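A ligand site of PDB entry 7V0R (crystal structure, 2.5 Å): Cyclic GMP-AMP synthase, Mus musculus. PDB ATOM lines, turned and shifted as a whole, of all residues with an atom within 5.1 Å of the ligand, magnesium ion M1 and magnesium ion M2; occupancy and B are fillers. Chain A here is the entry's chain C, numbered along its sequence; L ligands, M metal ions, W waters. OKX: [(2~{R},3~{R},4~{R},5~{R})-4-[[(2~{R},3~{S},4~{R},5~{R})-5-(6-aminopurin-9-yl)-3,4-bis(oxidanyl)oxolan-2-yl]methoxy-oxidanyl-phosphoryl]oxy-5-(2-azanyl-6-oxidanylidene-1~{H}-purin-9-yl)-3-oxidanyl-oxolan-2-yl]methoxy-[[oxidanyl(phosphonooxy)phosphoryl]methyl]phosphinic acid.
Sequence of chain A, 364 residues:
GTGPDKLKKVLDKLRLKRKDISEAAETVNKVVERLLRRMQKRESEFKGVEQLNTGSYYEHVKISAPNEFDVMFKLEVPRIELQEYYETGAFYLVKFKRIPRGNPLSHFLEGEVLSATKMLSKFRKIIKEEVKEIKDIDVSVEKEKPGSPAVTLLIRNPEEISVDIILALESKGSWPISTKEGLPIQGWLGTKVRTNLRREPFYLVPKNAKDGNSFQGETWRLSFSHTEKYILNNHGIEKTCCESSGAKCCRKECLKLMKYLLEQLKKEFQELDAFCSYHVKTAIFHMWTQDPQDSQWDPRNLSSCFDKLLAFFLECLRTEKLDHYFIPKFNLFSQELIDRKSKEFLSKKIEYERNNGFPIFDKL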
ATOM      1  N   GLY A  55     -13.347  31.556  -9.183  1.00  0.00           N
ATOM      2  CA  GLY A  55     -12.204  30.727  -8.872  1.00  0.00           C
ATOM      3  C   GLY A  55     -11.187  31.437  -8.007  1.00  0.00           C
ATOM      4  O   GLY A  55     -11.407  32.571  -7.565  1.00  0.00           O
ATOM      5  N   SER A  56     -10.050  30.764  -7.813  1.00  0.00           N
ATOM      6  CA  SER A  56      -9.030  31.086  -6.832  1.00  0.00           C
ATOM      7  C   SER A  56      -8.547  32.498  -6.867  1.00  0.00           C
ATOM      8  O   SER A  56      -8.451  33.132  -5.825  1.00  0.00           O
ATOM      9  CB  SER A  56      -7.814  30.229  -7.064  1.00  0.00           C
ATOM     10  OG  SER A  56      -8.106  28.943  -6.643  1.00  0.00           O
ATOM     11  N   GLU A  59     -11.033  34.753  -5.662  1.00  0.00           N
ATOM     12  CA  GLU A  59     -11.275  34.435  -4.254  1.00  0.00           C
ATOM     13  C   GLU A  59     -10.103  34.800  -3.323  1.00  0.00           C
ATOM     14  O   GLU A  59     -10.243  34.730  -2.111  1.00  0.00           O
ATOM     15  CB  GLU A  59     -11.610  32.949  -4.121  1.00  0.00           C
ATOM     16  CG  GLU A  59     -12.947  32.567  -4.763  1.00  0.00           C
ATOM     17  CD  GLU A  59     -13.119  31.076  -4.914  1.00  0.00           C
ATOM     18  OE1 GLU A  59     -12.146  30.311  -4.718  1.00  0.00           O
ATOM     19  OE2 GLU A  59     -14.271  30.674  -5.221  1.00  0.00           O
ATOM     20  N   VAL A  61      -7.408  33.018  -3.094  1.00  0.00           N
ATOM     21  CA  VAL A  61      -6.767  31.802  -2.601  1.00  0.00           C
ATOM     22  C   VAL A  61      -5.897  31.114  -3.680  1.00  0.00           C
ATOM     23  O   VAL A  61      -5.577  29.927  -3.579  1.00  0.00           O
ATOM     24  CB  VAL A  61      -7.789  30.828  -1.981  1.00  0.00           C
ATOM     25  CG1 VAL A  61      -8.284  31.401  -0.674  1.00  0.00           C
ATOM     26  CG2 VAL A  61      -8.947  30.554  -2.910  1.00  0.00           C
ATOM     27  N   LYS A  62      -5.500  31.863  -4.690  1.00  0.00           N
ATOM     28  CA  LYS A  62      -4.549  31.389  -5.685  1.00  0.00           C
ATOM     29  C   LYS A  62      -3.200  31.297  -5.033  1.00  0.00           C
ATOM     30  O   LYS A  62      -2.791  32.196  -4.334  1.00  0.00           O
ATOM     31  CB  LYS A  62      -4.492  32.328  -6.879  1.00  0.00           C
ATOM     32  CG  LYS A  62      -3.668  31.807  -8.027  1.00  0.00           C
ATOM     33  CD  LYS A  62      -4.362  30.656  -8.709  1.00  0.00           C
ATOM     34  CE  LYS A  62      -3.533  30.063  -9.826  1.00  0.00           C
ATOM     35  NZ  LYS A  62      -2.265  29.468  -9.340  1.00  0.00           N
ATOM     36  N   GLU A  68      -3.512  30.935 -13.453  1.00  0.00           N
ATOM     37  CA  GLU A  68      -4.751  30.235 -13.790  1.00  0.00           C
ATOM     38  C   GLU A  68      -5.916  31.148 -13.400  1.00  0.00           C
ATOM     39  O   GLU A  68      -6.006  31.569 -12.258  1.00  0.00           O
ATOM     40  CB  GLU A  68      -4.831  28.907 -13.021  1.00  0.00           C
ATOM     41  CG  GLU A  68      -5.388  27.718 -13.798  1.00  0.00           C
ATOM     42  CD  GLU A  68      -6.906  27.695 -13.959  1.00  0.00           C
ATOM     43  OE1 GLU A  68      -7.689  27.981 -13.001  1.00  0.00           O
ATOM     44  OE2 GLU A  68      -7.331  27.343 -15.087  1.00  0.00           O
ATOM     45  N   PHE A  69      -6.757  31.490 -14.394  1.00  0.00           N
ATOM     46  CA  PHE A  69      -7.851  32.440 -14.261  1.00  0.00           C
ATOM     47  C   PHE A  69      -9.134  31.803 -14.776  1.00  0.00           C
ATOM     48  O   PHE A  69      -9.150  31.178 -15.821  1.00  0.00           O
ATOM     49  CB  PHE A  69      -7.560  33.718 -15.072  1.00  0.00           C
ATOM     50  CG  PHE A  69      -6.386  34.534 -14.554  1.00  0.00           C
ATOM     51  CD1 PHE A  69      -5.109  34.171 -14.837  1.00  0.00           C
ATOM     52  CD2 PHE A  69      -6.605  35.674 -13.804  1.00  0.00           C
ATOM     53  CE1 PHE A  69      -4.037  34.908 -14.355  1.00  0.00           C
ATOM     54  CE2 PHE A  69      -5.540  36.427 -13.337  1.00  0.00           C
ATOM     55  CZ  PHE A  69      -4.259  36.038 -13.607  1.00  0.00           C
ATOM     56  N   ASP A  70     -10.229  31.957 -14.026  1.00  0.00           N
ATOM     57  CA  ASP A  70     -11.497  31.386 -14.431  1.00  0.00           C
ATOM     58  C   ASP A  70     -12.514  32.486 -14.636  1.00  0.00           C
ATOM     59  O   ASP A  70     -12.732  33.296 -13.747  1.00  0.00           O
ATOM     60  CB  ASP A  70     -11.982  30.371 -13.402  1.00  0.00           C
ATOM     61  CG  ASP A  70     -10.937  29.359 -13.049  1.00  0.00           C
ATOM     62  OD1 ASP A  70     -10.606  28.516 -13.890  1.00  0.00           O
ATOM     63  OD2 ASP A  70     -10.395  29.416 -11.936  1.00  0.00           O
ATOM     64  N   MET A  72     -16.469  33.274 -16.204  1.00  0.00           N
ATOM     65  CA  MET A  72     -17.758  32.827 -16.660  1.00  0.00           C
ATOM     66  C   MET A  72     -18.331  33.844 -17.637  1.00  0.00           C
ATOM     67  O   MET A  72     -18.408  35.018 -17.323  1.00  0.00           O
ATOM     68  CB  MET A  72     -18.701  32.643 -15.485  1.00  0.00           C
ATOM     69  CG  MET A  72     -18.853  31.197 -15.099  1.00  0.00           C
ATOM     70  SD  MET A  72     -19.940  30.867 -13.705  1.00  0.00           S
ATOM     71  CE  MET A  72     -21.493  31.501 -14.339  1.00  0.00           C
ATOM     72  N   GLY A 147     -15.142  16.493 -20.780  1.00  0.00           N
ATOM     73  CA  GLY A 147     -15.254  16.651 -19.335  1.00  0.00           C
ATOM     74  C   GLY A 147     -15.069  18.087 -18.857  1.00  0.00           C
ATOM     75  O   GLY A 147     -15.379  18.397 -17.704  1.00  0.00           O
ATOM     76  N   SER A 148     -14.572  18.961 -19.744  1.00  0.00           N
ATOM     77  CA  SER A 148     -14.462  20.386 -19.456  1.00  0.00           C
ATOM     78  C   SER A 148     -15.584  21.178 -20.109  1.00  0.00           C
ATOM     79  O   SER A 148     -15.837  21.059 -21.309  1.00  0.00           O
ATOM     80  CB  SER A 148     -13.146  20.958 -19.935  1.00  0.00           C
ATOM     81  OG  SER A 148     -13.147  22.337 -19.585  1.00  0.00           O
ATOM     82  N   PRO A 149     -16.257  22.062 -19.353  1.00  0.00           N
ATOM     83  CA  PRO A 149     -17.198  23.010 -19.934  1.00  0.00           C
ATOM     84  C   PRO A 149     -16.515  24.296 -20.422  1.00  0.00           C
ATOM     85  O   PRO A 149     -17.208  25.263 -20.732  1.00  0.00           O
ATOM     86  CB  PRO A 149     -18.078  23.310 -18.721  1.00  0.00           C
ATOM     87  CG  PRO A 149     -17.079  23.351 -17.596  1.00  0.00           C
ATOM     88  CD  PRO A 149     -16.106  22.228 -17.896  1.00  0.00           C
ATOM     89  N   ALA A 150     -15.179  24.290 -20.474  1.00  0.00           N
ATOM     90  CA  ALA A 150     -14.401  25.500 -20.649  1.00  0.00           C
ATOM     91  C   ALA A 150     -13.704  25.492 -21.981  1.00  0.00           C
ATOM     92  O   ALA A 150     -13.360  24.422 -22.487  1.00  0.00           O
ATOM     93  CB  ALA A 150     -13.380  25.614 -19.544  1.00  0.00           C
ATOM     94  N   ASP A 164      -9.631  29.813 -18.350  1.00  0.00           N
ATOM     95  CA  ASP A 164     -10.813  29.032 -18.686  1.00  0.00           C
ATOM     96  C   ASP A 164     -11.972  29.979 -18.934  1.00  0.00           C
ATOM     97  O   ASP A 164     -12.365  30.724 -18.051  1.00  0.00           O
ATOM     98  CB  ASP A 164     -11.130  28.052 -17.552  1.00  0.00           C
ATOM     99  CG  ASP A 164     -10.021  27.030 -17.330  1.00  0.00           C
ATOM    100  OD1 ASP A 164      -9.449  26.556 -18.322  1.00  0.00           O
ATOM    101  OD2 ASP A 164      -9.662  26.720 -16.152  1.00  0.00           O
ATOM    102  N   ILE A 166     -15.715  29.923 -19.456  1.00  0.00           N
ATOM    103  CA  ILE A 166     -16.756  28.971 -19.102  1.00  0.00           C
ATOM    104  C   ILE A 166     -18.097  29.524 -19.542  1.00  0.00           C
ATOM    105  O   ILE A 166     -18.536  30.603 -19.104  1.00  0.00           O
ATOM    106  CB  ILE A 166     -16.784  28.738 -17.582  1.00  0.00           C
ATOM    107  CG1 ILE A 166     -15.405  28.342 -17.080  1.00  0.00           C
ATOM    108  CG2 ILE A 166     -17.789  27.659 -17.233  1.00  0.00           C
ATOM    109  CD1 ILE A 166     -15.075  29.007 -15.755  1.00  0.00           C
ATOM    110  N   VAL A 205     -23.793  24.756 -16.687  1.00  0.00           N
ATOM    111  CA  VAL A 205     -22.521  24.824 -17.328  1.00  0.00           C
ATOM    112  C   VAL A 205     -22.434  23.536 -18.148  1.00  0.00           C
ATOM    113  O   VAL A 205     -22.876  22.475 -17.687  1.00  0.00           O
ATOM    114  CB  VAL A 205     -21.466  25.039 -16.192  1.00  0.00           C
ATOM    115  CG1 VAL A 205     -20.327  24.040 -16.212  1.00  0.00           C
ATOM    116  CG2 VAL A 205     -21.017  26.498 -16.157  1.00  0.00           C
ATOM    117  N   LYS A 207     -21.153  20.600 -18.911  1.00  0.00           N
ATOM    118  CA  LYS A 207     -20.186  19.553 -18.544  1.00  0.00           C
ATOM    119  C   LYS A 207     -20.681  18.183 -19.018  1.00  0.00           C
ATOM    120  O   LYS A 207     -21.830  17.805 -18.811  1.00  0.00           O
ATOM    121  CB  LYS A 207     -19.798  19.559 -17.053  1.00  0.00           C
ATOM    122  CG  LYS A 207     -18.434  18.912 -16.835  1.00  0.00           C
ATOM    123  CD  LYS A 207     -18.092  18.736 -15.375  1.00  0.00           C
ATOM    124  CE  LYS A 207     -16.715  18.110 -15.179  1.00  0.00           C
ATOM    125  NZ  LYS A 207     -16.159  18.440 -13.832  1.00  0.00           N
ATOM    126  N   ARG A 221     -24.528  20.967 -16.202  1.00  0.00           N
ATOM    127  CA  ARG A 221     -24.227  20.817 -14.760  1.00  0.00           C
ATOM    128  C   ARG A 221     -24.441  22.147 -14.013  1.00  0.00           C
ATOM    129  O   ARG A 221     -24.045  23.203 -14.535  1.00  0.00           O
ATOM    130  CB  ARG A 221     -22.810  20.306 -14.507  1.00  0.00           C
ATOM    131  CG  ARG A 221     -22.592  19.931 -13.045  1.00  0.00           C
ATOM    132  CD  ARG A 221     -21.269  19.280 -12.713  1.00  0.00           C
ATOM    133  NE  ARG A 221     -20.158  20.012 -13.313  1.00  0.00           N
ATOM    134  CZ  ARG A 221     -19.242  20.720 -12.646  1.00  0.00           C
ATOM    135  NH1 ARG A 221     -19.276  20.777 -11.324  1.00  0.00           N
ATOM    136  NH2 ARG A 221     -18.281  21.336 -13.295  1.00  0.00           N
ATOM    137  N   LEU A 222     -25.029  22.070 -12.814  1.00  0.00           N
ATOM    138  CA  LEU A 222     -25.177  23.220 -11.919  1.00  0.00           C
ATOM    139  C   LEU A 222     -23.814  23.732 -11.514  1.00  0.00           C
ATOM    140  O   LEU A 222     -22.899  22.954 -11.234  1.00  0.00           O
ATOM    141  CB  LEU A 222     -25.965  22.858 -10.664  1.00  0.00           C
ATOM    142  CG  LEU A 222     -27.427  22.490 -10.874  1.00  0.00           C
ATOM    143  CD1 LEU A 222     -27.939  21.720  -9.671  1.00  0.00           C
ATOM    144  CD2 LEU A 222     -28.249  23.752 -11.106  1.00  0.00           C
ATOM    145  N   SER A 223     -23.682  25.059 -11.532  1.00  0.00           N
ATOM    146  CA  SER A 223     -22.513  25.747 -11.047  1.00  0.00           C
ATOM    147  C   SER A 223     -22.962  26.783 -10.018  1.00  0.00           C
ATOM    148  O   SER A 223     -23.968  27.495 -10.216  1.00  0.00           O
ATOM    149  CB  SER A 223     -21.784  26.431 -12.189  1.00  0.00           C
ATOM    150  OG  SER A 223     -20.849  27.364 -11.697  1.00  0.00           O
ATOM    151  N   SER A 225     -20.298  28.759  -8.579  1.00  0.00           N
ATOM    152  CA  SER A 225     -19.052  29.502  -8.490  1.00  0.00           C
ATOM    153  C   SER A 225     -19.276  30.890  -7.941  1.00  0.00           C
ATOM    154  O   SER A 225     -18.431  31.393  -7.218  1.00  0.00           O
ATOM    155  CB  SER A 225     -18.442  29.698  -9.869  1.00  0.00           C
ATOM    156  OG  SER A 225     -18.030  28.493 -10.422  1.00  0.00           O
ATOM    157  N   LYS A 259      -4.625  22.949  -0.596  1.00  0.00           N
ATOM    158  CA  LYS A 259      -4.505  22.962  -2.054  1.00  0.00           C
ATOM    159  C   LYS A 259      -3.109  22.650  -2.531  1.00  0.00           C
ATOM    160  O   LYS A 259      -2.930  21.924  -3.511  1.00  0.00           O
ATOM    161  CB  LYS A 259      -4.895  24.317  -2.636  1.00  0.00           C
ATOM    162  CG  LYS A 259      -6.402  24.477  -2.724  1.00  0.00           C
ATOM    163  CD  LYS A 259      -6.748  25.930  -2.844  1.00  0.00           C
ATOM    164  CE  LYS A 259      -6.481  26.419  -4.237  1.00  0.00           C
ATOM    165  NZ  LYS A 259      -6.837  27.844  -4.221  1.00  0.00           N
ATOM    166  N   GLU A 263      -1.720  19.662  -4.923  1.00  0.00           N
ATOM    167  CA  GLU A 263      -0.925  19.992  -6.134  1.00  0.00           C
ATOM    168  C   GLU A 263       0.433  19.271  -6.152  1.00  0.00           C
ATOM    169  O   GLU A 263       0.830  18.702  -7.160  1.00  0.00           O
ATOM    170  CB  GLU A 263      -0.686  21.515  -6.264  1.00  0.00           C
ATOM    171  CG  GLU A 263      -1.747  22.313  -7.017  1.00  0.00           C
ATOM    172  CD  GLU A 263      -1.276  23.737  -7.383  1.00  0.00           C
ATOM    173  OE1 GLU A 263      -0.049  23.957  -7.592  1.00  0.00           O
ATOM    174  OE2 GLU A 263      -2.121  24.670  -7.441  1.00  0.00           O
ATOM    175  N   CYS A 276      -8.807  16.615  -7.476  1.00  0.00           N
ATOM    176  CA  CYS A 276      -8.695  17.986  -7.951  1.00  0.00           C
ATOM    177  C   CYS A 276      -8.942  18.939  -6.807  1.00  0.00           C
ATOM    178  O   CYS A 276      -9.454  18.547  -5.773  1.00  0.00           O
ATOM    179  CB  CYS A 276      -9.700  18.294  -9.063  1.00  0.00           C
ATOM    180  SG  CYS A 276     -11.433  18.246  -8.548  1.00  0.00           S
ATOM    181  N   SER A 277      -8.597  20.203  -7.004  1.00  0.00           N
ATOM    182  CA  SER A 277      -8.716  21.210  -5.976  1.00  0.00           C
ATOM    183  C   SER A 277     -10.162  21.406  -5.492  1.00  0.00           C
ATOM    184  O   SER A 277     -10.354  21.794  -4.358  1.00  0.00           O
ATOM    185  CB  SER A 277      -8.114  22.533  -6.433  1.00  0.00           C
ATOM    186  OG  SER A 277      -8.850  23.103  -7.491  1.00  0.00           O
ATOM    187  N   TYR A 278     -11.162  21.143  -6.332  1.00  0.00           N
ATOM    188  CA  TYR A 278     -12.592  21.329  -5.919  1.00  0.00           C
ATOM    189  C   TYR A 278     -12.894  20.379  -4.747  1.00  0.00           C
ATOM    190  O   TYR A 278     -13.761  20.735  -3.897  1.00  0.00           O
ATOM    191  CB  TYR A 278     -13.602  21.147  -7.066  1.00  0.00           C
ATOM    192  CG  TYR A 278     -14.965  21.674  -6.693  1.00  0.00           C
ATOM    193  CD1 TYR A 278     -15.193  23.039  -6.516  1.00  0.00           C
ATOM    194  CD2 TYR A 278     -16.032  20.814  -6.433  1.00  0.00           C
ATOM    195  CE1 TYR A 278     -16.435  23.537  -6.167  1.00  0.00           C
ATOM    196  CE2 TYR A 278     -17.286  21.299  -6.059  1.00  0.00           C
ATOM    197  CZ  TYR A 278     -17.488  22.669  -5.940  1.00  0.00           C
ATOM    198  OH  TYR A 278     -18.699  23.172  -5.558  1.00  0.00           O
ATOM    199  N   LYS A 281     -11.739  22.166  -1.674  1.00  0.00           N
ATOM    200  CA  LYS A 281     -12.602  23.318  -1.455  1.00  0.00           C
ATOM    201  C   LYS A 281     -13.919  22.914  -0.820  1.00  0.00           C
ATOM    202  O   LYS A 281     -14.359  23.534   0.159  1.00  0.00           O
ATOM    203  CB  LYS A 281     -12.906  24.019  -2.789  1.00  0.00           C
ATOM    204  CG  LYS A 281     -13.331  25.466  -2.636  1.00  0.00           C
ATOM    205  CD  LYS A 281     -13.794  25.991  -3.978  1.00  0.00           C
ATOM    206  CE  LYS A 281     -13.750  27.506  -4.060  1.00  0.00           C
ATOM    207  NZ  LYS A 281     -14.645  28.037  -5.122  1.00  0.00           N
ATOM    208  N   HIS A 324     -21.234  17.128  -2.325  1.00  0.00           N
ATOM    209  CA  HIS A 324     -21.258  18.460  -2.887  1.00  0.00           C
ATOM    210  C   HIS A 324     -21.928  19.369  -1.864  1.00  0.00           C
ATOM    211  O   HIS A 324     -22.981  19.018  -1.331  1.00  0.00           O
ATOM    212  CB  HIS A 324     -22.030  18.471  -4.202  1.00  0.00           C
ATOM    213  CG  HIS A 324     -21.744  19.653  -5.057  1.00  0.00           C
ATOM    214  ND1 HIS A 324     -22.226  20.915  -4.766  1.00  0.00           N
ATOM    215  CD2 HIS A 324     -21.017  19.783  -6.190  1.00  0.00           C
ATOM    216  CE1 HIS A 324     -21.806  21.764  -5.681  1.00  0.00           C
ATOM    217  NE2 HIS A 324     -21.058  21.096  -6.550  1.00  0.00           N
HETATM  218  N1  OKX L   1     -14.500  25.352 -10.982  1.00  0.00           N
HETATM  219  C1  OKX L   1     -14.897  24.097 -10.756  1.00  0.00           C
HETATM  220  N2  OKX L   1     -14.032  23.101 -10.873  1.00  0.00           N
HETATM  221  C2  OKX L   1     -14.598  21.897 -10.614  1.00  0.00           C
HETATM  222  C3  OKX L   1     -15.900  21.624 -10.256  1.00  0.00           C
HETATM  223  N3  OKX L   1     -16.082  20.264 -10.072  1.00  0.00           N
HETATM  224  C4  OKX L   1     -14.902  19.739 -10.317  1.00  0.00           C
HETATM  225  N4  OKX L   1     -13.968  20.686 -10.655  1.00  0.00           N
HETATM  226  C5  OKX L   1     -12.564  20.455 -10.976  1.00  0.00           C
HETATM  227  O1  OKX L   1     -11.794  20.969  -9.917  1.00  0.00           O
HETATM  228  C6  OKX L   1     -10.727  21.809 -10.420  1.00  0.00           C
HETATM  229  C7  OKX L   1     -10.985  23.230  -9.983  1.00  0.00           C
HETATM  230  O2  OKX L   1     -10.799  24.137 -11.101  1.00  0.00           O
HETATM  231  P1  OKX L   1     -10.835  25.710 -10.910  1.00  0.00           P
HETATM  232  O3  OKX L   1     -12.033  26.281 -11.616  1.00  0.00           O
HETATM  233  O4  OKX L   1      -9.504  26.298 -11.285  1.00  0.00           O
HETATM  234  C8  OKX L   1     -11.093  25.941  -9.129  1.00  0.00           C
HETATM  235  P2  OKX L   1     -10.194  27.332  -8.356  1.00  0.00           P
HETATM  236  O5  OKX L   1      -9.920  28.361  -9.415  1.00  0.00           O
HETATM  237  O6  OKX L   1     -11.010  27.791  -7.176  1.00  0.00           O
HETATM  238  O7  OKX L   1      -8.832  26.703  -7.836  1.00  0.00           O
HETATM  239  P3  OKX L   1      -7.376  26.509  -8.488  1.00  0.00           P
HETATM  240  O8  OKX L   1      -6.400  27.040  -7.480  1.00  0.00           O
HETATM  241  O9  OKX L   1      -7.373  27.305  -9.778  1.00  0.00           O
HETATM  242  O10 OKX L   1      -7.224  25.031  -8.727  1.00  0.00           O
HETATM  243  C9  OKX L   1     -10.678  21.555 -11.928  1.00  0.00           C
HETATM  244  O11 OKX L   1      -9.725  20.545 -12.235  1.00  0.00           O
HETATM  245  C10 OKX L   1     -12.102  21.129 -12.260  1.00  0.00           C
HETATM  246  O12 OKX L   1     -12.120  20.190 -13.323  1.00  0.00           O
HETATM  247  P4  OKX L   1     -13.241  20.627 -14.389  1.00  0.00           P
HETATM  248  O13 OKX L   1     -13.029  19.897 -15.681  1.00  0.00           O
HETATM  249  O14 OKX L   1     -14.600  20.560 -13.739  1.00  0.00           O
HETATM  250  O15 OKX L   1     -12.845  22.165 -14.593  1.00  0.00           O
HETATM  251  C11 OKX L   1     -12.447  22.638 -15.894  1.00  0.00           C
HETATM  252  C12 OKX L   1     -12.460  24.145 -15.868  1.00  0.00           C
HETATM  253  O16 OKX L   1     -13.787  24.590 -16.273  1.00  0.00           O
HETATM  254  C13 OKX L   1     -14.309  25.498 -15.336  1.00  0.00           C
HETATM  255  N5  OKX L   1     -15.348  24.824 -14.563  1.00  0.00           N
HETATM  256  C14 OKX L   1     -15.389  23.501 -14.200  1.00  0.00           C
HETATM  257  N6  OKX L   1     -16.454  23.189 -13.494  1.00  0.00           N
HETATM  258  C15 OKX L   1     -17.154  24.385 -13.388  1.00  0.00           C
HETATM  259  C16 OKX L   1     -18.369  24.717 -12.759  1.00  0.00           C
HETATM  260  N7  OKX L   1     -19.123  23.851 -12.105  1.00  0.00           N
HETATM  261  N8  OKX L   1     -18.782  26.002 -12.848  1.00  0.00           N
HETATM  262  C17 OKX L   1     -18.021  26.879 -13.513  1.00  0.00           C
HETATM  263  N9  OKX L   1     -16.867  26.681 -14.144  1.00  0.00           N
HETATM  264  C18 OKX L   1     -16.479  25.401 -14.041  1.00  0.00           C
HETATM  265  C19 OKX L   1     -13.141  26.000 -14.494  1.00  0.00           C
HETATM  266  O17 OKX L   1     -12.534  27.142 -15.055  1.00  0.00           O
HETATM  267  C20 OKX L   1     -12.210  24.779 -14.491  1.00  0.00           C
HETATM  268  O18 OKX L   1     -10.850  25.158 -14.343  1.00  0.00           O
HETATM  269  C21 OKX L   1     -16.818  22.696 -10.132  1.00  0.00           C
HETATM  270  O19 OKX L   1     -18.018  22.638  -9.819  1.00  0.00           O
HETATM  271  N10 OKX L   1     -16.209  23.923 -10.405  1.00  0.00           N
HETATM  272 MG    MG M   1      -8.804  28.235 -10.896  1.00  0.00          MG
HETATM  273 MG    MG M   2      -9.096  27.094 -13.769  1.00  0.00          MG
HETATM  274  O   HOH W   1      -7.879  30.237 -10.373  1.00  0.00           O
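Within 4 Å of magnesium ion M2: Glu 68, Asp 70 and Asp 164.
The nearest printed residue that does not touch magnesium ion M2 is Phe 69 (4.6 Å).
Magnesium ion M1 is bound by O5 of the ligand, O9 of the ligand, O4 of the ligand, OD2 of Asp 70, water W1 and OE1 of Glu 68.
OD2 of Asp 164 sits close to O18 of the ligand (2.7 Å).
The side-chain hydroxyl (OG) of Ser 56 lies within hydrogen-bond range of an oxygen (O7) of the ligand, 2.6 Å away.
NZ of Lys 207 is in salt-bridge range of O14 of the ligand (2.6 Å).
NH2 of Arg 221 is in salt-bridge range of O14 of the ligand.
OG of Ser 223 is in hydrogen-bond range of N8 of the ligand, 2.7 Å away.
O6 of the ligand sits at hydrogen-bond distance from N of Ser 56 (3.2 Å).
SG of Cys 276 sits at hydrogen-bond distance from O1 of the ligand (3.1 Å).
The side-chain amino group of Lys 259 is in salt-bridge range of an oxygen (O8) of the ligand (3.4 Å).
OG of Ser 277 sits at hydrogen-bond distance from O10 of the ligand (2.8 Å).
Water W1 lies within hydrogen-bond range of O of Glu 68 (3.0 Å) and N of Ser 56 (3.4 Å).
An oxygen (O13) of the ligand lies close to the backbone carbonyl oxygen (O) of Gly 147 (3.4 Å).
CA of Gly 55 touches O5 of the ligand (3.3 Å).
Glu 59 touches the ligand.
Ser 148 touches the ligand (OG to C11, 3.8 Å).
Pro 149 touches the ligand.
CB of Ala 150 touches O16 of the ligand (3.5 Å).
Ile 166 touches the ligand.
Leu 222 touches the ligand.
Ser 225 touches the ligand (OG to C17, 3.5 Å).
Tyr 278 touches the ligand.
Hydrophobic or aromatic side chains that line the ligand: Pro 149, Ala 150, Ile 166 and Tyr 278.
Within 4 Å of the ligand: Gly 55, Ser 56, Glu 59, Glu 68, Asp 70, Gly 147, Ser 148, Pro 149, Ala 150, Asp 164, Ile 166, Lys 207, Arg 221, Leu 222, Ser 223, Ser 225, Lys 259, Cys 276, Ser 277 and Tyr 278.
The nearest printed residue that does not touch the ligand is Val 205 (4.01 Å).
Within 4 Å of magnesium ion M1: Glu 68 and Asp 70.
The side-chain hydroxyl (OG) of Ser 56 is in hydrogen-bond range of the side-chain amino group (NZ) of Lys 259 (2.9 Å).
NZ of Lys 281 lies within salt-bridge range of OE2 of Glu 59.
The backbone carbonyl oxygen of Ser 56 sits at hydrogen-bond distance from the backbone NH of Lys 62 (3.4 Å).
OH of Tyr 278 sits at hydrogen-bond distance from NE2 of His 324, 3.3 Å away.
The backbone carbonyl oxygen of Arg 221 sits at hydrogen-bond distance from the backbone NH of Val 205 (2.7 Å).
The side-chain sulfur of Cys 276 sits close to the backbone NH of Tyr 278.
The backbone NH (N) of Val 61 lies within hydrogen-bond range of the backbone carbonyl oxygen (O) of Ser 56 (2.9 Å).
The side-chain amino group of Lys 259 sits at hydrogen-bond distance from the backbone carbonyl oxygen of Val 61 (2.5 Å).
Magnesium ion M2 is bound by the side-chain carboxylate (OE1) of Glu 68 (1.8 Å), the side-chain carboxylate (OD1) of Asp 70 (2.1 Å), the side-chain carboxylate (OE2) of Glu 68 (2.2 Å) and the side-chain carboxylate (OD2) of Asp 164 (2.5 Å).
Slightly farther from magnesium ion M2 lies an oxygen (O4) of the ligand (2.6 Å).
Slightly farther from magnesium ion M2 lies an oxygen (O18) of the ligand (2.7 Å).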
